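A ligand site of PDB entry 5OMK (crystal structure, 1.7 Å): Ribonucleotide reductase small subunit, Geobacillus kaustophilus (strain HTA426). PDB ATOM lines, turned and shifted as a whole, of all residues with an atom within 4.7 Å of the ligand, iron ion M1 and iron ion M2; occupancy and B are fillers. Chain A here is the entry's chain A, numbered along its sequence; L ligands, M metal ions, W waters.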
ATOM      1  N   LEU A  75     -18.237 -31.421 -23.025  1.00  0.00           N
ATOM      2  CA  LEU A  75     -17.282 -31.613 -21.936  1.00  0.00           C
ATOM      3  C   LEU A  75     -16.053 -32.379 -22.421  1.00  0.00           C
ATOM      4  O   LEU A  75     -14.925 -32.011 -22.077  1.00  0.00           O
ATOM      5  CB  LEU A  75     -17.945 -32.329 -20.767  1.00  0.00           C
ATOM      6  CG  LEU A  75     -17.154 -32.394 -19.458  1.00  0.00           C
ATOM      7  CD1 LEU A  75     -16.831 -30.975 -18.979  1.00  0.00           C
ATOM      8  CD2 LEU A  75     -17.951 -33.189 -18.368  1.00  0.00           C
ATOM      9  N   GLY A  78     -13.957 -30.131 -24.507  1.00  0.00           N
ATOM     10  CA  GLY A  78     -13.122 -29.270 -23.687  1.00  0.00           C
ATOM     11  C   GLY A  78     -11.920 -30.008 -23.138  1.00  0.00           C
ATOM     12  O   GLY A  78     -10.804 -29.478 -23.126  1.00  0.00           O
ATOM     13  N   PHE A  79     -12.113 -31.251 -22.679  1.00  0.00           N
ATOM     14  CA  PHE A  79     -10.996 -31.978 -22.093  1.00  0.00           C
ATOM     15  C   PHE A  79      -9.957 -32.372 -23.134  1.00  0.00           C
ATOM     16  O   PHE A  79      -8.762 -32.177 -22.907  1.00  0.00           O
ATOM     17  CB  PHE A  79     -11.480 -33.190 -21.314  1.00  0.00           C
ATOM     18  CG  PHE A  79     -11.625 -32.923 -19.834  1.00  0.00           C
ATOM     19  CD1 PHE A  79     -10.508 -32.861 -19.018  1.00  0.00           C
ATOM     20  CD2 PHE A  79     -12.862 -32.737 -19.260  1.00  0.00           C
ATOM     21  CE1 PHE A  79     -10.626 -32.607 -17.661  1.00  0.00           C
ATOM     22  CE2 PHE A  79     -12.993 -32.501 -17.901  1.00  0.00           C
ATOM     23  CZ  PHE A  79     -11.881 -32.431 -17.095  1.00  0.00           C
ATOM     24  N   GLY A  82      -7.959 -29.597 -24.094  1.00  0.00           N
ATOM     25  CA  GLY A  82      -7.201 -29.170 -22.938  1.00  0.00           C
ATOM     26  C   GLY A  82      -5.963 -30.022 -22.709  1.00  0.00           C
ATOM     27  O   GLY A  82      -4.880 -29.490 -22.459  1.00  0.00           O
ATOM     28  N   GLU A  83      -6.132 -31.355 -22.761  1.00  0.00           N
ATOM     29  CA  GLU A  83      -5.021 -32.285 -22.559  1.00  0.00           C
ATOM     30  C   GLU A  83      -3.959 -32.097 -23.629  1.00  0.00           C
ATOM     31  O   GLU A  83      -2.754 -32.106 -23.340  1.00  0.00           O
ATOM     32  CB  GLU A  83      -5.478 -33.735 -22.583  1.00  0.00           C
ATOM     33  CG  GLU A  83      -6.612 -34.116 -21.665  1.00  0.00           C
ATOM     34  CD  GLU A  83      -6.338 -33.928 -20.172  1.00  0.00           C
ATOM     35  OE1 GLU A  83      -7.320 -33.937 -19.390  1.00  0.00           O
ATOM     36  OE2 GLU A  83      -5.156 -33.768 -19.769  1.00  0.00           O
ATOM     37  N   VAL A  86      -2.030 -28.703 -23.031  1.00  0.00           N
ATOM     38  CA  VAL A  86      -1.045 -28.771 -21.933  1.00  0.00           C
ATOM     39  C   VAL A  86       0.104 -29.745 -22.234  1.00  0.00           C
ATOM     40  O   VAL A  86       1.232 -29.541 -21.775  1.00  0.00           O
ATOM     41  CB  VAL A  86      -1.722 -29.113 -20.583  1.00  0.00           C
ATOM     42  CG1 VAL A  86      -2.709 -28.043 -20.222  1.00  0.00           C
ATOM     43  CG2 VAL A  86      -2.382 -30.479 -20.611  1.00  0.00           C
ATOM     44  N   PHE A 112       5.148 -35.162 -15.368  1.00  0.00           N
ATOM     45  CA  PHE A 112       4.062 -34.253 -15.736  1.00  0.00           C
ATOM     46  C   PHE A 112       3.716 -34.386 -17.230  1.00  0.00           C
ATOM     47  O   PHE A 112       2.559 -34.609 -17.606  1.00  0.00           O
ATOM     48  CB  PHE A 112       4.521 -32.830 -15.371  1.00  0.00           C
ATOM     49  CG  PHE A 112       3.437 -31.774 -15.281  1.00  0.00           C
ATOM     50  CD1 PHE A 112       3.527 -30.782 -14.316  1.00  0.00           C
ATOM     51  CD2 PHE A 112       2.405 -31.708 -16.184  1.00  0.00           C
ATOM     52  CE1 PHE A 112       2.581 -29.783 -14.210  1.00  0.00           C
ATOM     53  CE2 PHE A 112       1.456 -30.693 -16.093  1.00  0.00           C
ATOM     54  CZ  PHE A 112       1.544 -29.732 -15.121  1.00  0.00           C
ATOM     55  N   GLU A 116       0.278 -36.017 -19.071  1.00  0.00           N
ATOM     56  CA  GLU A 116      -0.609 -35.331 -20.012  1.00  0.00           C
ATOM     57  C   GLU A 116      -0.736 -36.093 -21.306  1.00  0.00           C
ATOM     58  O   GLU A 116      -1.838 -36.142 -21.880  1.00  0.00           O
ATOM     59  CB  GLU A 116      -0.118 -33.900 -20.259  1.00  0.00           C
ATOM     60  CG  GLU A 116      -0.043 -33.018 -19.013  1.00  0.00           C
ATOM     61  CD  GLU A 116      -1.395 -32.768 -18.313  1.00  0.00           C
ATOM     62  OE1 GLU A 116      -1.424 -31.904 -17.423  1.00  0.00           O
ATOM     63  OE2 GLU A 116      -2.431 -33.368 -18.671  1.00  0.00           O
ATOM     64  N   HIS A 119      -3.203 -38.580 -20.734  1.00  0.00           N
ATOM     65  CA  HIS A 119      -4.543 -38.003 -20.695  1.00  0.00           C
ATOM     66  C   HIS A 119      -5.086 -37.785 -22.100  1.00  0.00           C
ATOM     67  O   HIS A 119      -6.268 -38.060 -22.362  1.00  0.00           O
ATOM     68  CB  HIS A 119      -4.572 -36.662 -19.963  1.00  0.00           C
ATOM     69  CG  HIS A 119      -4.110 -36.733 -18.546  1.00  0.00           C
ATOM     70  ND1 HIS A 119      -3.976 -35.605 -17.744  1.00  0.00           N
ATOM     71  CD2 HIS A 119      -3.715 -37.781 -17.798  1.00  0.00           C
ATOM     72  CE1 HIS A 119      -3.560 -35.984 -16.555  1.00  0.00           C
ATOM     73  NE2 HIS A 119      -3.344 -37.289 -16.567  1.00  0.00           N
ATOM     74  N   TYR A 145     -13.409 -20.162 -24.398  1.00  0.00           N
ATOM     75  CA  TYR A 145     -12.534 -21.311 -24.339  1.00  0.00           C
ATOM     76  C   TYR A 145     -11.286 -21.087 -25.199  1.00  0.00           C
ATOM     77  O   TYR A 145     -10.148 -21.362 -24.762  1.00  0.00           O
ATOM     78  CB  TYR A 145     -13.292 -22.559 -24.794  1.00  0.00           C
ATOM     79  CG  TYR A 145     -12.458 -23.818 -24.703  1.00  0.00           C
ATOM     80  CD1 TYR A 145     -12.539 -24.665 -23.594  1.00  0.00           C
ATOM     81  CD2 TYR A 145     -11.590 -24.144 -25.737  1.00  0.00           C
ATOM     82  CE1 TYR A 145     -11.769 -25.798 -23.522  1.00  0.00           C
ATOM     83  CE2 TYR A 145     -10.819 -25.274 -25.682  1.00  0.00           C
ATOM     84  CZ  TYR A 145     -10.884 -26.091 -24.550  1.00  0.00           C
ATOM     85  OH  TYR A 145     -10.124 -27.209 -24.499  1.00  0.00           O
ATOM     86  N   PHE A 149      -7.341 -21.488 -24.106  1.00  0.00           N
ATOM     87  CA  PHE A 149      -6.580 -22.648 -24.577  1.00  0.00           C
ATOM     88  C   PHE A 149      -5.894 -22.444 -25.920  1.00  0.00           C
ATOM     89  O   PHE A 149      -4.803 -22.996 -26.133  1.00  0.00           O
ATOM     90  CB  PHE A 149      -7.515 -23.851 -24.661  1.00  0.00           C
ATOM     91  CG  PHE A 149      -7.880 -24.382 -23.310  1.00  0.00           C
ATOM     92  CD1 PHE A 149      -7.022 -25.276 -22.661  1.00  0.00           C
ATOM     93  CD2 PHE A 149      -9.072 -23.998 -22.660  1.00  0.00           C
ATOM     94  CE1 PHE A 149      -7.323 -25.748 -21.407  1.00  0.00           C
ATOM     95  CE2 PHE A 149      -9.376 -24.501 -21.400  1.00  0.00           C
ATOM     96  CZ  PHE A 149      -8.487 -25.392 -20.772  1.00  0.00           C
ATOM     97  N   VAL A 180      -6.080 -23.413 -15.713  1.00  0.00           N
ATOM     98  CA  VAL A 180      -6.454 -24.531 -16.575  1.00  0.00           C
ATOM     99  C   VAL A 180      -6.614 -25.819 -15.747  1.00  0.00           C
ATOM    100  O   VAL A 180      -7.615 -26.539 -15.881  1.00  0.00           O
ATOM    101  CB  VAL A 180      -5.406 -24.683 -17.706  1.00  0.00           C
ATOM    102  CG1 VAL A 180      -5.401 -26.076 -18.325  1.00  0.00           C
ATOM    103  CG2 VAL A 180      -5.645 -23.596 -18.767  1.00  0.00           C
ATOM    104  N   GLU A 181      -5.623 -26.147 -14.930  1.00  0.00           N
ATOM    105  CA  GLU A 181      -5.674 -27.371 -14.114  1.00  0.00           C
ATOM    106  C   GLU A 181      -6.467 -27.151 -12.827  1.00  0.00           C
ATOM    107  O   GLU A 181      -7.441 -27.860 -12.531  1.00  0.00           O
ATOM    108  CB  GLU A 181      -4.253 -27.834 -13.783  1.00  0.00           C
ATOM    109  CG  GLU A 181      -3.491 -28.248 -14.991  1.00  0.00           C
ATOM    110  CD  GLU A 181      -2.096 -28.729 -14.688  1.00  0.00           C
ATOM    111  OE1 GLU A 181      -1.396 -28.073 -13.897  1.00  0.00           O
ATOM    112  OE2 GLU A 181      -1.718 -29.790 -15.202  1.00  0.00           O
ATOM    113  N   LEU A 184     -10.304 -25.210 -13.933  1.00  0.00           N
ATOM    114  CA  LEU A 184     -11.144 -25.828 -14.967  1.00  0.00           C
ATOM    115  C   LEU A 184     -11.077 -27.352 -14.929  1.00  0.00           C
ATOM    116  O   LEU A 184     -12.123 -28.012 -14.835  1.00  0.00           O
ATOM    117  CB  LEU A 184     -10.768 -25.284 -16.333  1.00  0.00           C
ATOM    118  CG  LEU A 184     -11.158 -23.837 -16.632  1.00  0.00           C
ATOM    119  CD1 LEU A 184     -10.517 -23.342 -17.931  1.00  0.00           C
ATOM    120  CD2 LEU A 184     -12.679 -23.689 -16.725  1.00  0.00           C
ATOM    121  N   ALA A 185      -9.891 -27.950 -14.969  1.00  0.00           N
ATOM    122  CA  ALA A 185      -9.807 -29.417 -14.944  1.00  0.00           C
ATOM    123  C   ALA A 185     -10.489 -30.000 -13.708  1.00  0.00           C
ATOM    124  O   ALA A 185     -11.241 -30.991 -13.788  1.00  0.00           O
ATOM    125  CB  ALA A 185      -8.338 -29.887 -14.993  1.00  0.00           C
ATOM    126  N   SER A 187     -12.845 -28.772 -11.825  1.00  0.00           N
ATOM    127  CA  SER A 187     -14.298 -28.645 -11.918  1.00  0.00           C
ATOM    128  C   SER A 187     -14.835 -29.624 -12.949  1.00  0.00           C
ATOM    129  O   SER A 187     -15.905 -30.191 -12.777  1.00  0.00           O
ATOM    130  CB  SER A 187     -14.676 -27.208 -12.276  1.00  0.00           C
ATOM    131  OG  SER A 187     -14.148 -26.309 -11.316  1.00  0.00           O
ATOM    132  N   GLY A 188     -14.080 -29.862 -14.018  1.00  0.00           N
ATOM    133  CA  GLY A 188     -14.513 -30.862 -14.982  1.00  0.00           C
ATOM    134  C   GLY A 188     -14.613 -32.255 -14.395  1.00  0.00           C
ATOM    135  O   GLY A 188     -15.513 -33.014 -14.753  1.00  0.00           O
ATOM    136  N   TYR A 189     -13.648 -32.642 -13.571  1.00  0.00           N
ATOM    137  CA  TYR A 189     -13.702 -33.957 -12.940  1.00  0.00           C
ATOM    138  C   TYR A 189     -14.943 -34.061 -12.090  1.00  0.00           C
ATOM    139  O   TYR A 189     -15.676 -35.060 -12.129  1.00  0.00           O
ATOM    140  CB  TYR A 189     -12.478 -34.195 -12.053  1.00  0.00           C
ATOM    141  CG  TYR A 189     -11.161 -34.104 -12.789  1.00  0.00           C
ATOM    142  CD1 TYR A 189     -11.052 -34.575 -14.075  1.00  0.00           C
ATOM    143  CD2 TYR A 189     -10.029 -33.540 -12.168  1.00  0.00           C
ATOM    144  CE1 TYR A 189      -9.872 -34.518 -14.755  1.00  0.00           C
ATOM    145  CE2 TYR A 189      -8.848 -33.454 -12.837  1.00  0.00           C
ATOM    146  CZ  TYR A 189      -8.758 -33.942 -14.144  1.00  0.00           C
ATOM    147  OH  TYR A 189      -7.571 -33.887 -14.847  1.00  0.00           O
ATOM    148  N   THR A 191     -17.692 -32.326 -12.400  1.00  0.00           N
ATOM    149  CA  THR A 191     -18.874 -32.337 -13.271  1.00  0.00           C
ATOM    150  C   THR A 191     -19.128 -33.726 -13.835  1.00  0.00           C
ATOM    151  O   THR A 191     -20.270 -34.219 -13.790  1.00  0.00           O
ATOM    152  CB  THR A 191     -18.712 -31.295 -14.378  1.00  0.00           C
ATOM    153  OG1 THR A 191     -18.526 -30.004 -13.799  1.00  0.00           O
ATOM    154  CG2 THR A 191     -19.894 -31.234 -15.290  1.00  0.00           C
ATOM    155  N   GLU A 216      -3.600 -35.071 -11.435  1.00  0.00           N
ATOM    156  CA  GLU A 216      -3.721 -33.621 -11.400  1.00  0.00           C
ATOM    157  C   GLU A 216      -3.229 -33.043 -10.107  1.00  0.00           C
ATOM    158  O   GLU A 216      -2.731 -31.921 -10.086  1.00  0.00           O
ATOM    159  CB  GLU A 216      -5.182 -33.186 -11.602  1.00  0.00           C
ATOM    160  CG  GLU A 216      -5.336 -31.826 -12.181  1.00  0.00           C
ATOM    161  CD  GLU A 216      -4.882 -31.805 -13.614  1.00  0.00           C
ATOM    162  OE1 GLU A 216      -5.651 -32.305 -14.484  1.00  0.00           O
ATOM    163  OE2 GLU A 216      -3.717 -31.390 -13.845  1.00  0.00           O
ATOM    164  N   HIS A 219       0.306 -32.117 -10.557  1.00  0.00           N
ATOM    165  CA  HIS A 219       0.438 -30.972 -11.456  1.00  0.00           C
ATOM    166  C   HIS A 219       0.160 -29.668 -10.722  1.00  0.00           C
ATOM    167  O   HIS A 219       0.899 -28.681 -10.842  1.00  0.00           O
ATOM    168  CB  HIS A 219      -0.544 -31.139 -12.650  1.00  0.00           C
ATOM    169  CG  HIS A 219      -0.336 -32.405 -13.400  1.00  0.00           C
ATOM    170  ND1 HIS A 219      -1.095 -32.759 -14.504  1.00  0.00           N
ATOM    171  CD2 HIS A 219       0.514 -33.439 -13.172  1.00  0.00           C
ATOM    172  CE1 HIS A 219      -0.700 -33.954 -14.927  1.00  0.00           C
ATOM    173  NE2 HIS A 219       0.277 -34.376 -14.143  1.00  0.00           N
ATOM    174  N   TYR A 255     -16.783 -19.553 -20.263  1.00  0.00           N
ATOM    175  CA  TYR A 255     -16.868 -20.899 -20.798  1.00  0.00           C
ATOM    176  C   TYR A 255     -17.844 -21.736 -19.972  1.00  0.00           C
ATOM    177  O   TYR A 255     -18.642 -22.509 -20.524  1.00  0.00           O
ATOM    178  CB  TYR A 255     -15.477 -21.525 -20.812  1.00  0.00           C
ATOM    179  CG  TYR A 255     -15.454 -22.970 -21.244  1.00  0.00           C
ATOM    180  CD1 TYR A 255     -15.953 -23.353 -22.478  1.00  0.00           C
ATOM    181  CD2 TYR A 255     -14.905 -23.948 -20.423  1.00  0.00           C
ATOM    182  CE1 TYR A 255     -15.924 -24.705 -22.884  1.00  0.00           C
ATOM    183  CE2 TYR A 255     -14.862 -25.304 -20.828  1.00  0.00           C
ATOM    184  CZ  TYR A 255     -15.361 -25.659 -22.051  1.00  0.00           C
ATOM    185  OH  TYR A 255     -15.345 -26.981 -22.477  1.00  0.00           O
ATOM    186  N   VAL A 256     -17.781 -21.617 -18.655  1.00  0.00           N
ATOM    187  CA  VAL A 256     -18.695 -22.372 -17.788  1.00  0.00           C
ATOM    188  C   VAL A 256     -20.137 -22.023 -18.126  1.00  0.00           C
ATOM    189  O   VAL A 256     -20.986 -22.896 -18.264  1.00  0.00           O
ATOM    190  CB  VAL A 256     -18.363 -22.115 -16.310  1.00  0.00           C
ATOM    191  CG1 VAL A 256     -19.456 -22.677 -15.401  1.00  0.00           C
ATOM    192  CG2 VAL A 256     -17.043 -22.764 -15.928  1.00  0.00           C
ATOM    193  N   LEU A 259     -21.212 -23.770 -21.345  1.00  0.00           N
ATOM    194  CA  LEU A 259     -21.527 -25.183 -21.184  1.00  0.00           C
ATOM    195  C   LEU A 259     -22.843 -25.372 -20.434  1.00  0.00           C
ATOM    196  O   LEU A 259     -23.591 -26.309 -20.728  1.00  0.00           O
ATOM    197  CB  LEU A 259     -20.431 -25.897 -20.422  1.00  0.00           C
ATOM    198  CG  LEU A 259     -19.091 -26.017 -21.126  1.00  0.00           C
ATOM    199  CD1 LEU A 259     -18.167 -26.702 -20.135  1.00  0.00           C
ATOM    200  CD2 LEU A 259     -19.220 -26.810 -22.413  1.00  0.00           C
ATOM    201  N   THR A 260     -23.089 -24.533 -19.426  1.00  0.00           N
ATOM    202  CA  THR A 260     -24.346 -24.601 -18.700  1.00  0.00           C
ATOM    203  C   THR A 260     -25.527 -24.317 -19.630  1.00  0.00           C
ATOM    204  O   THR A 260     -26.531 -25.038 -19.607  1.00  0.00           O
ATOM    205  CB  THR A 260     -24.327 -23.593 -17.561  1.00  0.00           C
ATOM    206  OG1 THR A 260     -23.357 -24.005 -16.601  1.00  0.00           O
ATOM    207  CG2 THR A 260     -25.725 -23.517 -16.892  1.00  0.00           C
ATOM    208  N   TYR A 279     -26.906 -27.182 -12.111  1.00  0.00           N
ATOM    209  CA  TYR A 279     -25.921 -26.305 -12.737  1.00  0.00           C
ATOM    210  C   TYR A 279     -25.512 -25.166 -11.811  1.00  0.00           C
ATOM    211  O   TYR A 279     -24.352 -24.757 -11.803  1.00  0.00           O
ATOM    212  CB  TYR A 279     -26.448 -25.763 -14.065  1.00  0.00           C
ATOM    213  CG  TYR A 279     -26.526 -26.838 -15.095  1.00  0.00           C
ATOM    214  CD1 TYR A 279     -25.378 -27.391 -15.622  1.00  0.00           C
ATOM    215  CD2 TYR A 279     -27.751 -27.334 -15.525  1.00  0.00           C
ATOM    216  CE1 TYR A 279     -25.430 -28.400 -16.552  1.00  0.00           C
ATOM    217  CE2 TYR A 279     -27.817 -28.345 -16.468  1.00  0.00           C
ATOM    218  CZ  TYR A 279     -26.648 -28.873 -16.977  1.00  0.00           C
ATOM    219  OH  TYR A 279     -26.692 -29.881 -17.901  1.00  0.00           O
ATOM    220  N   LEU A 282     -22.742 -26.665  -9.840  1.00  0.00           N
ATOM    221  CA  LEU A 282     -21.515 -26.774 -10.613  1.00  0.00           C
ATOM    222  C   LEU A 282     -20.860 -25.408 -10.749  1.00  0.00           C
ATOM    223  O   LEU A 282     -19.646 -25.273 -10.582  1.00  0.00           O
ATOM    224  CB  LEU A 282     -21.806 -27.373 -11.985  1.00  0.00           C
ATOM    225  CG  LEU A 282     -22.332 -28.808 -12.022  1.00  0.00           C
ATOM    226  CD1 LEU A 282     -22.681 -29.216 -13.444  1.00  0.00           C
ATOM    227  CD2 LEU A 282     -21.347 -29.794 -11.386  1.00  0.00           C
ATOM    228  N   VAL A 286     -16.943 -24.188  -9.383  1.00  0.00           N
ATOM    229  CA  VAL A 286     -15.916 -23.473 -10.144  1.00  0.00           C
ATOM    230  C   VAL A 286     -15.437 -22.258  -9.371  1.00  0.00           C
ATOM    231  O   VAL A 286     -14.231 -22.032  -9.238  1.00  0.00           O
ATOM    232  CB  VAL A 286     -16.453 -23.064 -11.535  1.00  0.00           C
ATOM    233  CG1 VAL A 286     -15.429 -22.212 -12.280  1.00  0.00           C
ATOM    234  CG2 VAL A 286     -16.782 -24.274 -12.344  1.00  0.00           C
HETATM  235  C1  LIG L   1      -4.795 -30.853 -17.791  1.00  0.00           C
HETATM  236  O1  LIG L   1      -4.995 -31.922 -18.401  1.00  0.00           O
HETATM  237  O2  LIG L   1      -3.859 -30.581 -16.947  1.00  0.00           O
HETATM  238  C2  LIG L   1      -5.798 -29.695 -18.121  1.00  0.00           C
HETATM  239  C3  LIG L   1      -7.047 -30.085 -18.816  1.00  0.00           C
HETATM  240  C4  LIG L   1      -8.032 -28.938 -19.040  1.00  0.00           C
HETATM  241  C5  LIG L   1      -9.473 -29.383 -19.316  1.00  0.00           C
HETATM  242  C6  LIG L   1     -10.383 -28.264 -19.734  1.00  0.00           C
HETATM  243  C7  LIG L   1     -11.846 -28.636 -19.947  1.00  0.00           C
HETATM  244  C8  LIG L   1     -12.511 -28.918 -18.680  1.00  0.00           C
HETATM  245  C9  LIG L   1     -13.997 -28.749 -18.709  1.00  0.00           C
HETATM  246  C10 LIG L   1     -14.447 -27.662 -17.727  1.00  0.00           C
HETATM  247  C11 LIG L   1     -15.756 -27.951 -17.127  1.00  0.00           C
HETATM  248  C12 LIG L   1     -16.123 -26.974 -16.011  1.00  0.00           C
HETATM  249  C13 LIG L   1     -17.474 -27.329 -15.384  1.00  0.00           C
HETATM  250  C14 LIG L   1     -18.682 -26.561 -15.945  1.00  0.00           C
HETATM  251  C15 LIG L   1     -20.052 -27.133 -15.529  1.00  0.00           C
HETATM  252  C16 LIG L   1     -21.047 -27.343 -16.701  1.00  0.00           C
HETATM  253 FE    FE M   1      -2.586 -31.566 -15.689  1.00  0.00          FE
HETATM  254 FE    FE M   2      -4.342 -33.590 -17.916  1.00  0.00          FE
HETATM  255  O   HOH W   1      -3.743 -33.216 -15.993  1.00  0.00           O
HETATM  256  O   HOH W   2      -6.383 -33.970 -17.142  1.00  0.00           O
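CD1 of Leu 75 touches C9 of the ligand, at 3.6 Å.
Gly 78 touches the ligand.
CD1 of Phe 79 touches C5 of the ligand (3.6 Å).
Gly 82 touches the ligand.
Val 86 touches the ligand (CG2 to O1, 3.7 Å).
Phe 149 touches the ligand.
Val 180 touches the ligand (CG1 to C2, 3.6 Å).
Leu 184 touches the ligand (O to C10, 3.7 Å).
Gly 188 touches the ligand (CA to C11, 3.8 Å).
OG1 of Thr 191 touches C13 of the ligand, 3.3 Å away.
CE2 of Tyr 255 touches C10 of the ligand, 3.9 Å away.
CG1 of Val 256 touches C14 of the ligand, at 3.998 Å.
CD1 of Leu 282 touches C15 of the ligand, 3.9 Å away.
The nearest printed residue that does not touch the ligand is Ser 187 (4.01 Å).
Four residues have an atom within 4 Å of iron ion M2: Glu 83, Glu 116, His 119 and Glu 216.
The nearest printed residue that does not touch iron ion M2 is Tyr 189 (4.5 Å).
Iron ion M1 is bound by OE2 of Glu 181 (2.0 Å), water W1 (2.0 Å), O2 of the ligand (2.0 Å), OE1 of Glu 116 (2.1 Å), OE2 of Glu 216 (2.2 Å) and ND1 of His 219 (2.2 Å).
The nearest printed residue that does not touch iron ion M1 is Phe 112 (4.2 Å).
The side-chain hydroxyl (OH) of Tyr 189 sits at hydrogen-bond distance from the side-chain carboxylate (OE1) of Glu 216 (2.5 Å).
The side-chain hydroxyl of Thr 191 sits at hydrogen-bond distance from the backbone carbonyl oxygen of Ser 187, 2.8 Å away.
The side-chain hydroxyl of Tyr 145 is in hydrogen-bond range of the backbone carbonyl oxygen of Gly 78, 2.7 Å away.
The backbone carbonyl oxygen (O) of Val 180 lies within hydrogen-bond range of the backbone NH (N) of Ala 185 (2.8 Å).
OH of Tyr 145 lies within hydrogen-bond range of N of Gly 82, at 3.2 Å.
The side-chain hydroxyl (OG1) of Thr 260 is in hydrogen-bond range of the backbone carbonyl oxygen (O) of Val 256, 3.1 Å away.
Iron ion M2 is bound by O1 of the ligand, OE2 of Glu 83, water W1, ND1 of His 119, OE2 of Glu 116 and water W2.
Water W2 lies within hydrogen-bond range of the side-chain carboxylate (OE1) of Glu 83 (2.4 Å), the side-chain hydroxyl (OH) of Tyr 189 (2.6 Å) and the side-chain carboxylate (OE1) of Glu 216 (3.2 Å).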
